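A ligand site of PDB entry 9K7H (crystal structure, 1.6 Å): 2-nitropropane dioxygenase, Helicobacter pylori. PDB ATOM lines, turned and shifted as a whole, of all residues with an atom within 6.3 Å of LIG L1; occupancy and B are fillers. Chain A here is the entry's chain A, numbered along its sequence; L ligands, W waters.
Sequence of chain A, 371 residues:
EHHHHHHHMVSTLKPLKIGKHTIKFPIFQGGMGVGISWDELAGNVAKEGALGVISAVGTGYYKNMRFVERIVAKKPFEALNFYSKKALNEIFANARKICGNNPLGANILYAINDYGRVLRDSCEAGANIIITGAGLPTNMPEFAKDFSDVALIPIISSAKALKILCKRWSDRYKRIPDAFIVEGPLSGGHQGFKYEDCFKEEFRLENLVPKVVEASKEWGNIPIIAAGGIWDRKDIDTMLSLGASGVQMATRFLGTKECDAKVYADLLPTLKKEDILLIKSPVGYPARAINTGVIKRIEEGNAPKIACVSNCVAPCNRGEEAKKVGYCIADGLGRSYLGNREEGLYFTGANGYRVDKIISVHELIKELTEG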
ATOM      1  N   ASN A 113     -23.562 -17.022   0.226  1.00  0.00           N
ATOM      2  CA  ASN A 113     -24.462 -17.255   1.347  1.00  0.00           C
ATOM      3  C   ASN A 113     -24.077 -16.366   2.516  1.00  0.00           C
ATOM      4  O   ASN A 113     -22.909 -15.980   2.661  1.00  0.00           O
ATOM      5  CB  ASN A 113     -24.412 -18.727   1.770  1.00  0.00           C
ATOM      6  CG  ASN A 113     -25.179 -19.616   0.833  1.00  0.00           C
ATOM      7  OD1 ASN A 113     -26.319 -19.301   0.455  1.00  0.00           O
ATOM      8  ND2 ASN A 113     -24.557 -20.733   0.419  1.00  0.00           N
ATOM      9  N   PRO A 282     -19.689 -22.273 -10.738  1.00  0.00           N
ATOM     10  CA  PRO A 282     -20.878 -22.644  -9.949  1.00  0.00           C
ATOM     11  C   PRO A 282     -21.698 -21.448  -9.508  1.00  0.00           C
ATOM     12  O   PRO A 282     -22.844 -21.639  -9.075  1.00  0.00           O
ATOM     13  CB  PRO A 282     -20.294 -23.380  -8.737  1.00  0.00           C
ATOM     14  CG  PRO A 282     -18.846 -23.631  -9.045  1.00  0.00           C
ATOM     15  CD  PRO A 282     -18.428 -22.632 -10.066  1.00  0.00           C
ATOM     16  N   VAL A 283     -21.140 -20.229  -9.559  1.00  0.00           N
ATOM     17  CA  VAL A 283     -21.879 -19.030  -9.178  1.00  0.00           C
ATOM     18  C   VAL A 283     -22.869 -18.597 -10.251  1.00  0.00           C
ATOM     19  O   VAL A 283     -23.745 -17.769  -9.983  1.00  0.00           O
ATOM     20  CB  VAL A 283     -20.888 -17.893  -8.852  1.00  0.00           C
ATOM     21  CG1 VAL A 283     -21.580 -16.687  -8.170  1.00  0.00           C
ATOM     22  CG2 VAL A 283     -19.753 -18.410  -7.964  1.00  0.00           C
ATOM     23  N   ILE A 306     -15.803 -33.539  -5.807  1.00  0.00           N
ATOM     24  CA  ILE A 306     -16.718 -32.473  -5.399  1.00  0.00           C
ATOM     25  C   ILE A 306     -17.647 -33.004  -4.325  1.00  0.00           C
ATOM     26  O   ILE A 306     -18.371 -33.987  -4.528  1.00  0.00           O
ATOM     27  CB  ILE A 306     -17.517 -31.909  -6.586  1.00  0.00           C
ATOM     28  CG1 ILE A 306     -16.584 -31.243  -7.589  1.00  0.00           C
ATOM     29  CG2 ILE A 306     -18.651 -30.972  -6.102  1.00  0.00           C
ATOM     30  CD1 ILE A 306     -17.071 -31.285  -8.997  1.00  0.00           C
ATOM     31  N   ALA A 307     -17.657 -32.321  -3.195  1.00  0.00           N
ATOM     32  CA  ALA A 307     -18.593 -32.601  -2.112  1.00  0.00           C
ATOM     33  C   ALA A 307     -18.628 -31.317  -1.303  1.00  0.00           C
ATOM     34  O   ALA A 307     -17.639 -30.999  -0.625  1.00  0.00           O
ATOM     35  CB  ALA A 307     -18.144 -33.790  -1.272  1.00  0.00           C
ATOM     36  N   CYS A 308     -19.718 -30.583  -1.421  1.00  0.00           N
ATOM     37  CA  CYS A 308     -19.848 -29.266  -0.806  1.00  0.00           C
ATOM     38  C   CYS A 308     -19.600 -29.333   0.694  1.00  0.00           C
ATOM     39  O   CYS A 308     -20.347 -29.993   1.428  1.00  0.00           O
ATOM     40  CB  CYS A 308     -21.236 -28.688  -1.098  1.00  0.00           C
ATOM     41  SG  CYS A 308     -21.527 -27.006  -0.491  1.00  0.00           S
ATOM     42  N   VAL A 309     -18.560 -28.647   1.133  1.00  0.00           N
ATOM     43  CA  VAL A 309     -18.229 -28.496   2.535  1.00  0.00           C
ATOM     44  C   VAL A 309     -18.459 -27.057   3.004  1.00  0.00           C
ATOM     45  O   VAL A 309     -19.147 -26.813   3.989  1.00  0.00           O
ATOM     46  CB  VAL A 309     -16.776 -28.945   2.808  1.00  0.00           C
ATOM     47  CG1 VAL A 309     -16.337 -28.553   4.227  1.00  0.00           C
ATOM     48  CG2 VAL A 309     -16.616 -30.433   2.603  1.00  0.00           C
ATOM     49  N   SER A 310     -17.898 -26.086   2.268  1.00  0.00           N
ATOM     50  CA  SER A 310     -17.893 -24.691   2.701  1.00  0.00           C
ATOM     51  C   SER A 310     -19.178 -23.946   2.392  1.00  0.00           C
ATOM     52  O   SER A 310     -19.410 -22.874   2.967  1.00  0.00           O
ATOM     53  CB  SER A 310     -16.718 -23.941   2.063  1.00  0.00           C
ATOM     54  OG  SER A 310     -15.449 -24.488   2.410  1.00  0.00           O
ATOM     55  N   ASN A 311     -20.020 -24.476   1.485  1.00  0.00           N
ATOM     56  CA  ASN A 311     -21.322 -23.889   1.136  1.00  0.00           C
ATOM     57  C   ASN A 311     -21.200 -22.410   0.786  1.00  0.00           C
ATOM     58  O   ASN A 311     -21.919 -21.554   1.321  1.00  0.00           O
ATOM     59  CB  ASN A 311     -22.334 -24.109   2.262  1.00  0.00           C
ATOM     60  CG  ASN A 311     -23.758 -23.771   1.835  1.00  0.00           C
ATOM     61  OD1 ASN A 311     -24.072 -23.825   0.646  1.00  0.00           O
ATOM     62  ND2 ASN A 311     -24.614 -23.449   2.786  1.00  0.00           N
ATOM     63  N   CYS A 312     -20.337 -22.109  -0.192  1.00  0.00           N
ATOM     64  CA  CYS A 312     -19.889 -20.733  -0.364  1.00  0.00           C
ATOM     65  C   CYS A 312     -20.953 -19.818  -1.008  1.00  0.00           C
ATOM     66  O   CYS A 312     -21.098 -18.669  -0.603  1.00  0.00           O
ATOM     67  CB  CYS A 312     -18.557 -20.719  -1.135  1.00  0.00           C
ATOM     68  SG  CYS A 312     -18.605 -21.240  -2.884  1.00  0.00           S
ATOM     69  N   VAL A 313     -21.692 -20.291  -2.024  1.00  0.00           N
ATOM     70  CA  VAL A 313     -22.546 -19.373  -2.801  1.00  0.00           C
ATOM     71  C   VAL A 313     -23.940 -19.952  -2.989  1.00  0.00           C
ATOM     72  O   VAL A 313     -24.108 -21.146  -3.268  1.00  0.00           O
ATOM     73  CB  VAL A 313     -21.919 -19.004  -4.175  1.00  0.00           C
ATOM     74  CG1 VAL A 313     -20.602 -18.256  -3.985  1.00  0.00           C
ATOM     75  CG2 VAL A 313     -21.691 -20.228  -5.074  1.00  0.00           C
ATOM     76  N   ALA A 314     -24.945 -19.097  -2.858  1.00  0.00           N
ATOM     77  CA  ALA A 314     -26.329 -19.562  -3.017  1.00  0.00           C
ATOM     78  C   ALA A 314     -26.612 -20.210  -4.370  1.00  0.00           C
ATOM     79  O   ALA A 314     -27.273 -21.271  -4.383  1.00  0.00           O
ATOM     80  CB  ALA A 314     -27.274 -18.380  -2.742  1.00  0.00           C
ATOM     81  N   CYS A 316     -25.171 -22.128  -6.308  1.00  0.00           N
ATOM     82  CA  CYS A 316     -24.674 -23.481  -6.540  1.00  0.00           C
ATOM     83  C   CYS A 316     -25.616 -24.550  -5.992  1.00  0.00           C
ATOM     84  O   CYS A 316     -25.602 -25.681  -6.494  1.00  0.00           O
ATOM     85  CB  CYS A 316     -23.282 -23.628  -5.925  1.00  0.00           C
ATOM     86  SG  CYS A 316     -22.516 -25.288  -6.102  1.00  0.00           S
ATOM     87  N   ASN A 317     -26.415 -24.223  -4.983  1.00  0.00           N
ATOM     88  CA  ASN A 317     -27.296 -25.185  -4.320  1.00  0.00           C
ATOM     89  C   ASN A 317     -26.497 -26.388  -3.813  1.00  0.00           C
ATOM     90  O   ASN A 317     -26.703 -27.531  -4.222  1.00  0.00           O
ATOM     91  CB  ASN A 317     -28.463 -25.602  -5.234  1.00  0.00           C
ATOM     92  CG  ASN A 317     -29.407 -26.535  -4.539  1.00  0.00           C
ATOM     93  OD1 ASN A 317     -29.638 -26.405  -3.342  1.00  0.00           O
ATOM     94  ND2 ASN A 317     -29.945 -27.513  -5.268  1.00  0.00           N
ATOM     95  N   ARG A 318     -25.582 -26.106  -2.888  1.00  0.00           N
ATOM     96  CA  ARG A 318     -24.827 -27.125  -2.142  1.00  0.00           C
ATOM     97  C   ARG A 318     -24.175 -28.182  -3.046  1.00  0.00           C
ATOM     98  O   ARG A 318     -24.155 -29.368  -2.715  1.00  0.00           O
ATOM     99  CB  ARG A 318     -25.706 -27.790  -1.094  1.00  0.00           C
ATOM    100  CG  ARG A 318     -26.219 -26.804  -0.014  1.00  0.00           C
ATOM    101  CD  ARG A 318     -26.566 -27.563   1.259  1.00  0.00           C
ATOM    102  NE  ARG A 318     -26.972 -26.669   2.332  1.00  0.00           N
ATOM    103  CZ  ARG A 318     -26.197 -26.319   3.346  1.00  0.00           C
ATOM    104  NH1 ARG A 318     -24.955 -26.783   3.447  1.00  0.00           N
ATOM    105  NH2 ARG A 318     -26.661 -25.486   4.269  1.00  0.00           N
ATOM    106  N   GLY A 319     -23.643 -27.752  -4.191  1.00  0.00           N
ATOM    107  CA  GLY A 319     -22.886 -28.630  -5.062  1.00  0.00           C
ATOM    108  C   GLY A 319     -23.583 -29.024  -6.335  1.00  0.00           C
ATOM    109  O   GLY A 319     -22.935 -29.582  -7.232  1.00  0.00           O
ATOM    110  N   GLU A 320     -24.872 -28.709  -6.477  1.00  0.00           N
ATOM    111  CA  GLU A 320     -25.586 -29.009  -7.723  1.00  0.00           C
ATOM    112  C   GLU A 320     -24.855 -28.446  -8.925  1.00  0.00           C
ATOM    113  O   GLU A 320     -24.601 -29.150  -9.913  1.00  0.00           O
ATOM    114  CB  GLU A 320     -26.987 -28.442  -7.701  1.00  0.00           C
ATOM    115  CG  GLU A 320     -27.690 -28.751  -9.016  1.00  0.00           C
ATOM    116  CD  GLU A 320     -29.075 -28.164  -9.093  1.00  0.00           C
ATOM    117  OE1 GLU A 320     -29.515 -27.511  -8.133  1.00  0.00           O
ATOM    118  OE2 GLU A 320     -29.723 -28.380 -10.144  1.00  0.00           O
ATOM    119  N   GLU A 321     -24.503 -27.152  -8.863  1.00  0.00           N
ATOM    120  CA  GLU A 321     -23.925 -26.547 -10.056  1.00  0.00           C
ATOM    121  C   GLU A 321     -22.436 -26.839 -10.162  1.00  0.00           C
ATOM    122  O   GLU A 321     -21.929 -26.920 -11.281  1.00  0.00           O
ATOM    123  CB  GLU A 321     -24.182 -25.041 -10.085  1.00  0.00           C
ATOM    124  CG  GLU A 321     -25.647 -24.629  -9.977  1.00  0.00           C
ATOM    125  CD  GLU A 321     -26.602 -25.267 -11.000  1.00  0.00           C
ATOM    126  OE1 GLU A 321     -26.161 -25.803 -12.042  1.00  0.00           O
ATOM    127  OE2 GLU A 321     -27.831 -25.220 -10.746  1.00  0.00           O
ATOM    128  N   ALA A 322     -21.735 -26.976  -9.031  1.00  0.00           N
ATOM    129  CA  ALA A 322     -20.317 -27.342  -9.085  1.00  0.00           C
ATOM    130  C   ALA A 322     -20.135 -28.677  -9.786  1.00  0.00           C
ATOM    131  O   ALA A 322     -19.225 -28.837 -10.610  1.00  0.00           O
ATOM    132  CB  ALA A 322     -19.710 -27.390  -7.679  1.00  0.00           C
ATOM    133  N   LYS A 323     -20.991 -29.659  -9.471  1.00  0.00           N
ATOM    134  CA  LYS A 323     -20.909 -30.950 -10.140  1.00  0.00           C
ATOM    135  C   LYS A 323     -21.128 -30.805 -11.645  1.00  0.00           C
ATOM    136  O   LYS A 323     -20.430 -31.427 -12.449  1.00  0.00           O
ATOM    137  CB  LYS A 323     -21.904 -31.931  -9.510  1.00  0.00           C
ATOM    138  CG  LYS A 323     -21.479 -32.446  -8.113  1.00  0.00           C
ATOM    139  CD  LYS A 323     -22.643 -32.833  -7.214  1.00  0.00           C
ATOM    140  CE  LYS A 323     -22.197 -33.336  -5.819  1.00  0.00           C
ATOM    141  NZ  LYS A 323     -22.041 -32.311  -4.705  1.00  0.00           N
ATOM    142  N   TYR A 327     -16.196 -28.181 -11.170  1.00  0.00           N
ATOM    143  CA  TYR A 327     -15.266 -27.829 -10.100  1.00  0.00           C
ATOM    144  C   TYR A 327     -16.005 -27.003  -9.049  1.00  0.00           C
ATOM    145  O   TYR A 327     -17.006 -26.347  -9.337  1.00  0.00           O
ATOM    146  CB  TYR A 327     -14.063 -27.052 -10.654  1.00  0.00           C
ATOM    147  CG  TYR A 327     -14.425 -25.657 -11.086  1.00  0.00           C
ATOM    148  CD1 TYR A 327     -14.351 -24.579 -10.189  1.00  0.00           C
ATOM    149  CD2 TYR A 327     -14.833 -25.391 -12.388  1.00  0.00           C
ATOM    150  CE1 TYR A 327     -14.696 -23.304 -10.581  1.00  0.00           C
ATOM    151  CE2 TYR A 327     -15.152 -24.113 -12.796  1.00  0.00           C
ATOM    152  CZ  TYR A 327     -15.078 -23.072 -11.882  1.00  0.00           C
ATOM    153  OH  TYR A 327     -15.427 -21.788 -12.260  1.00  0.00           O
ATOM    154  N   CYS A 328     -15.469 -27.060  -7.817  1.00  0.00           N
ATOM    155  CA  CYS A 328     -15.897 -26.258  -6.678  1.00  0.00           C
ATOM    156  C   CYS A 328     -15.023 -25.016  -6.542  1.00  0.00           C
ATOM    157  O   CYS A 328     -13.805 -25.139  -6.375  1.00  0.00           O
ATOM    158  CB  CYS A 328     -15.819 -27.095  -5.395  1.00  0.00           C
ATOM    159  SG  CYS A 328     -16.077 -26.146  -3.834  1.00  0.00           S
ATOM    160  N   ILE A 329     -15.647 -23.842  -6.570  1.00  0.00           N
ATOM    161  CA  ILE A 329     -14.857 -22.610  -6.589  1.00  0.00           C
ATOM    162  C   ILE A 329     -14.200 -22.338  -5.223  1.00  0.00           C
ATOM    163  O   ILE A 329     -13.031 -21.938  -5.171  1.00  0.00           O
ATOM    164  CB  ILE A 329     -15.727 -21.439  -7.092  1.00  0.00           C
ATOM    165  CG1 ILE A 329     -14.842 -20.237  -7.438  1.00  0.00           C
ATOM    166  CG2 ILE A 329     -16.803 -21.104  -6.093  1.00  0.00           C
ATOM    167  CD1 ILE A 329     -15.518 -19.268  -8.389  1.00  0.00           C
ATOM    168  N   ALA A 330     -14.918 -22.590  -4.116  1.00  0.00           N
ATOM    169  CA  ALA A 330     -14.338 -22.424  -2.778  1.00  0.00           C
ATOM    170  C   ALA A 330     -13.104 -23.312  -2.586  1.00  0.00           C
ATOM    171  O   ALA A 330     -12.055 -22.845  -2.119  1.00  0.00           O
ATOM    172  CB  ALA A 330     -15.387 -22.723  -1.705  1.00  0.00           C
ATOM    173  N   ASP A 331     -13.233 -24.600  -2.921  1.00  0.00           N
ATOM    174  CA  ASP A 331     -12.125 -25.541  -2.756  1.00  0.00           C
ATOM    175  C   ASP A 331     -10.934 -25.124  -3.603  1.00  0.00           C
ATOM    176  O   ASP A 331      -9.775 -25.193  -3.170  1.00  0.00           O
ATOM    177  CB  ASP A 331     -12.523 -26.959  -3.159  1.00  0.00           C
ATOM    178  CG  ASP A 331     -13.552 -27.593  -2.228  1.00  0.00           C
ATOM    179  OD1 ASP A 331     -13.898 -27.014  -1.170  1.00  0.00           O
ATOM    180  OD2 ASP A 331     -13.970 -28.717  -2.562  1.00  0.00           O
HETATM  181 FE1  LIG L   1     -20.371 -25.717  -2.053  1.00  0.00          FE
HETATM  182 FE2  LIG L   1     -20.742 -25.082  -4.630  1.00  0.00          FE
HETATM  183 FE3  LIG L   1     -18.247 -25.580  -3.761  1.00  0.00          FE
HETATM  184 FE4  LIG L   1     -19.428 -23.332  -3.036  1.00  0.00          FE
HETATM  185  S1  LIG L   1     -18.858 -23.979  -5.200  1.00  0.00           S
HETATM  186  S2  LIG L   1     -18.393 -24.749  -1.584  1.00  0.00           S
HETATM  187  S3  LIG L   1     -21.592 -23.913  -2.797  1.00  0.00           S
HETATM  188  S4  LIG L   1     -19.926 -27.078  -3.888  1.00  0.00           S
HETATM  189  C1  LG2 L   2     -16.095 -14.276 -10.028  1.00  0.00           C
HETATM  190  C2  LG2 L   2     -17.367 -15.696 -11.436  1.00  0.00           C
HETATM  191  C3  LG2 L   2     -15.675 -15.788  -6.557  1.00  0.00           C
HETATM  192  C4  LG2 L   2     -16.765 -16.620  -6.336  1.00  0.00           C
HETATM  193  C5  LG2 L   2     -16.833 -17.385  -5.174  1.00  0.00           C
HETATM  194  C6  LG2 L   2     -14.675 -15.718  -5.618  1.00  0.00           C
HETATM  195  C7  LG2 L   2     -13.790 -12.181 -12.032  1.00  0.00           C
HETATM  196  C8  LG2 L   2     -12.865 -13.184 -11.788  1.00  0.00           C
HETATM  197  C9  LG2 L   2     -11.795 -13.354 -12.661  1.00  0.00           C
HETATM  198  C10 LG2 L   2     -11.629 -12.513 -13.748  1.00  0.00           C
HETATM  199  C11 LG2 L   2     -12.551 -11.506 -13.978  1.00  0.00           C
HETATM  200  C12 LG2 L   2     -12.404 -10.556 -15.154  1.00  0.00           C
HETATM  201  C13 LG2 L   2     -13.617 -11.346 -13.119  1.00  0.00           C
HETATM  202  C14 LG2 L   2     -16.695 -14.503 -11.263  1.00  0.00           C
HETATM  203  C15 LG2 L   2     -17.408 -16.615 -10.402  1.00  0.00           C
HETATM  204  C16 LG2 L   2     -16.184 -15.223  -9.027  1.00  0.00           C
HETATM  205  C17 LG2 L   2     -15.800 -17.301  -4.255  1.00  0.00           C
HETATM  206  C18 LG2 L   2     -14.734 -16.469  -4.469  1.00  0.00           C
HETATM  207  N1  LG2 L   2     -14.955 -11.914 -11.202  1.00  0.00           N
HETATM  208  N2  LG2 L   2     -16.821 -16.343  -9.249  1.00  0.00           N
HETATM  209  N3  LG2 L   2     -15.549 -14.954  -7.744  1.00  0.00           N
HETATM  210  O1  LG2 L   2     -16.016 -11.953  -8.752  1.00  0.00           O
HETATM  211  O2  LG2 L   2     -11.467 -10.696 -15.976  1.00  0.00           O
HETATM  212  O3  LG2 L   2     -13.204  -9.600 -15.292  1.00  0.00           O
HETATM  213  O4  LG2 L   2     -13.951 -12.970  -9.032  1.00  0.00           O
HETATM  214  S1  LG2 L   2     -15.217 -12.721  -9.721  1.00  0.00           S
HETATM  215 CL1  LG2 L   2     -15.821 -18.255  -2.766  1.00  0.00          CL
HETATM  216 CL2  LG2 L   2     -13.282 -14.658  -5.886  1.00  0.00          CL
HETATM  217  O   HOH W   1     -16.631 -27.007  -0.326  1.00  0.00           O
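An iron atom (FE3) of LIG L1 is bound by the side-chain sulfur (SG) of Cys 328. N of Cys 312 lies close to S3 of LIG L1, at 3.4 Å. SG of Cys 312 binds FE4 of LIG L1 (2.3 Å). An iron atom (FE2) of LIG L1 is bound by the side-chain sulfur of Cys 316, at 2.3 Å. The side-chain sulfur of Cys 308 binds an iron atom (FE1) of LIG L1, at 2.3 Å. The backbone NH of Asn 311 lies close to a sulfur (S2) of LIG L1. The backbone NH (N) of Ile 329 sits close to a sulfur (S1) of LIG L1. S4 of LIG L1 sits close to N of Gly 319 (3.8 Å). N of Val 313 lies close to S3 of LIG L1, 3.7 Å away.
The backbone NH (N) of Ala 330 sits close to the side-chain sulfur (SG) of Cys 328. SG of Cys 328 lies close to N of Asp 331. O of Cys 312 is in hydrogen-bond range of N of Asn 113. SG of Cys 316 lies close to N of Gly 319, at 3.3 Å. The backbone NH (N) of Ala 322 lies close to the side-chain sulfur (SG) of Cys 316 (3.5 Å). N of Glu 321 is in hydrogen-bond range of O of Cys 316. SG of Cys 308 sits close to N of Asn 311 (3.5 Å). The side-chain amide nitrogen (ND2) of Asn 311 sits close to the guanidinium group (NH2) of Arg 318, 3.2 Å away.
Merely in contact with LIG L1: Pro 282 (3.9 Å), Ala 322 (3.8 Å) and Ala 330 (3.6 Å). Hydrophobic or aromatic side chains within 4 Å of LIG L1: Pro 282, Ala 322, Ile 329 and Ala 330. 11 residues have an atom within 4 Å of LIG L1: Pro 282, Cys 308, Asn 311, Cys 312, Val 313, Cys 316, Gly 319, Ala 322, Cys 328, Ile 329 and Ala 330.
Water W1 lies within hydrogen-bond range of the side-chain carboxylate of Asp 331 (2.9 Å), the backbone NH of Val 309 (2.9 Å), the backbone NH of Ser 310 (3.0 Å) and a sulfur (S2) of LIG L1 (3.1 Å).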
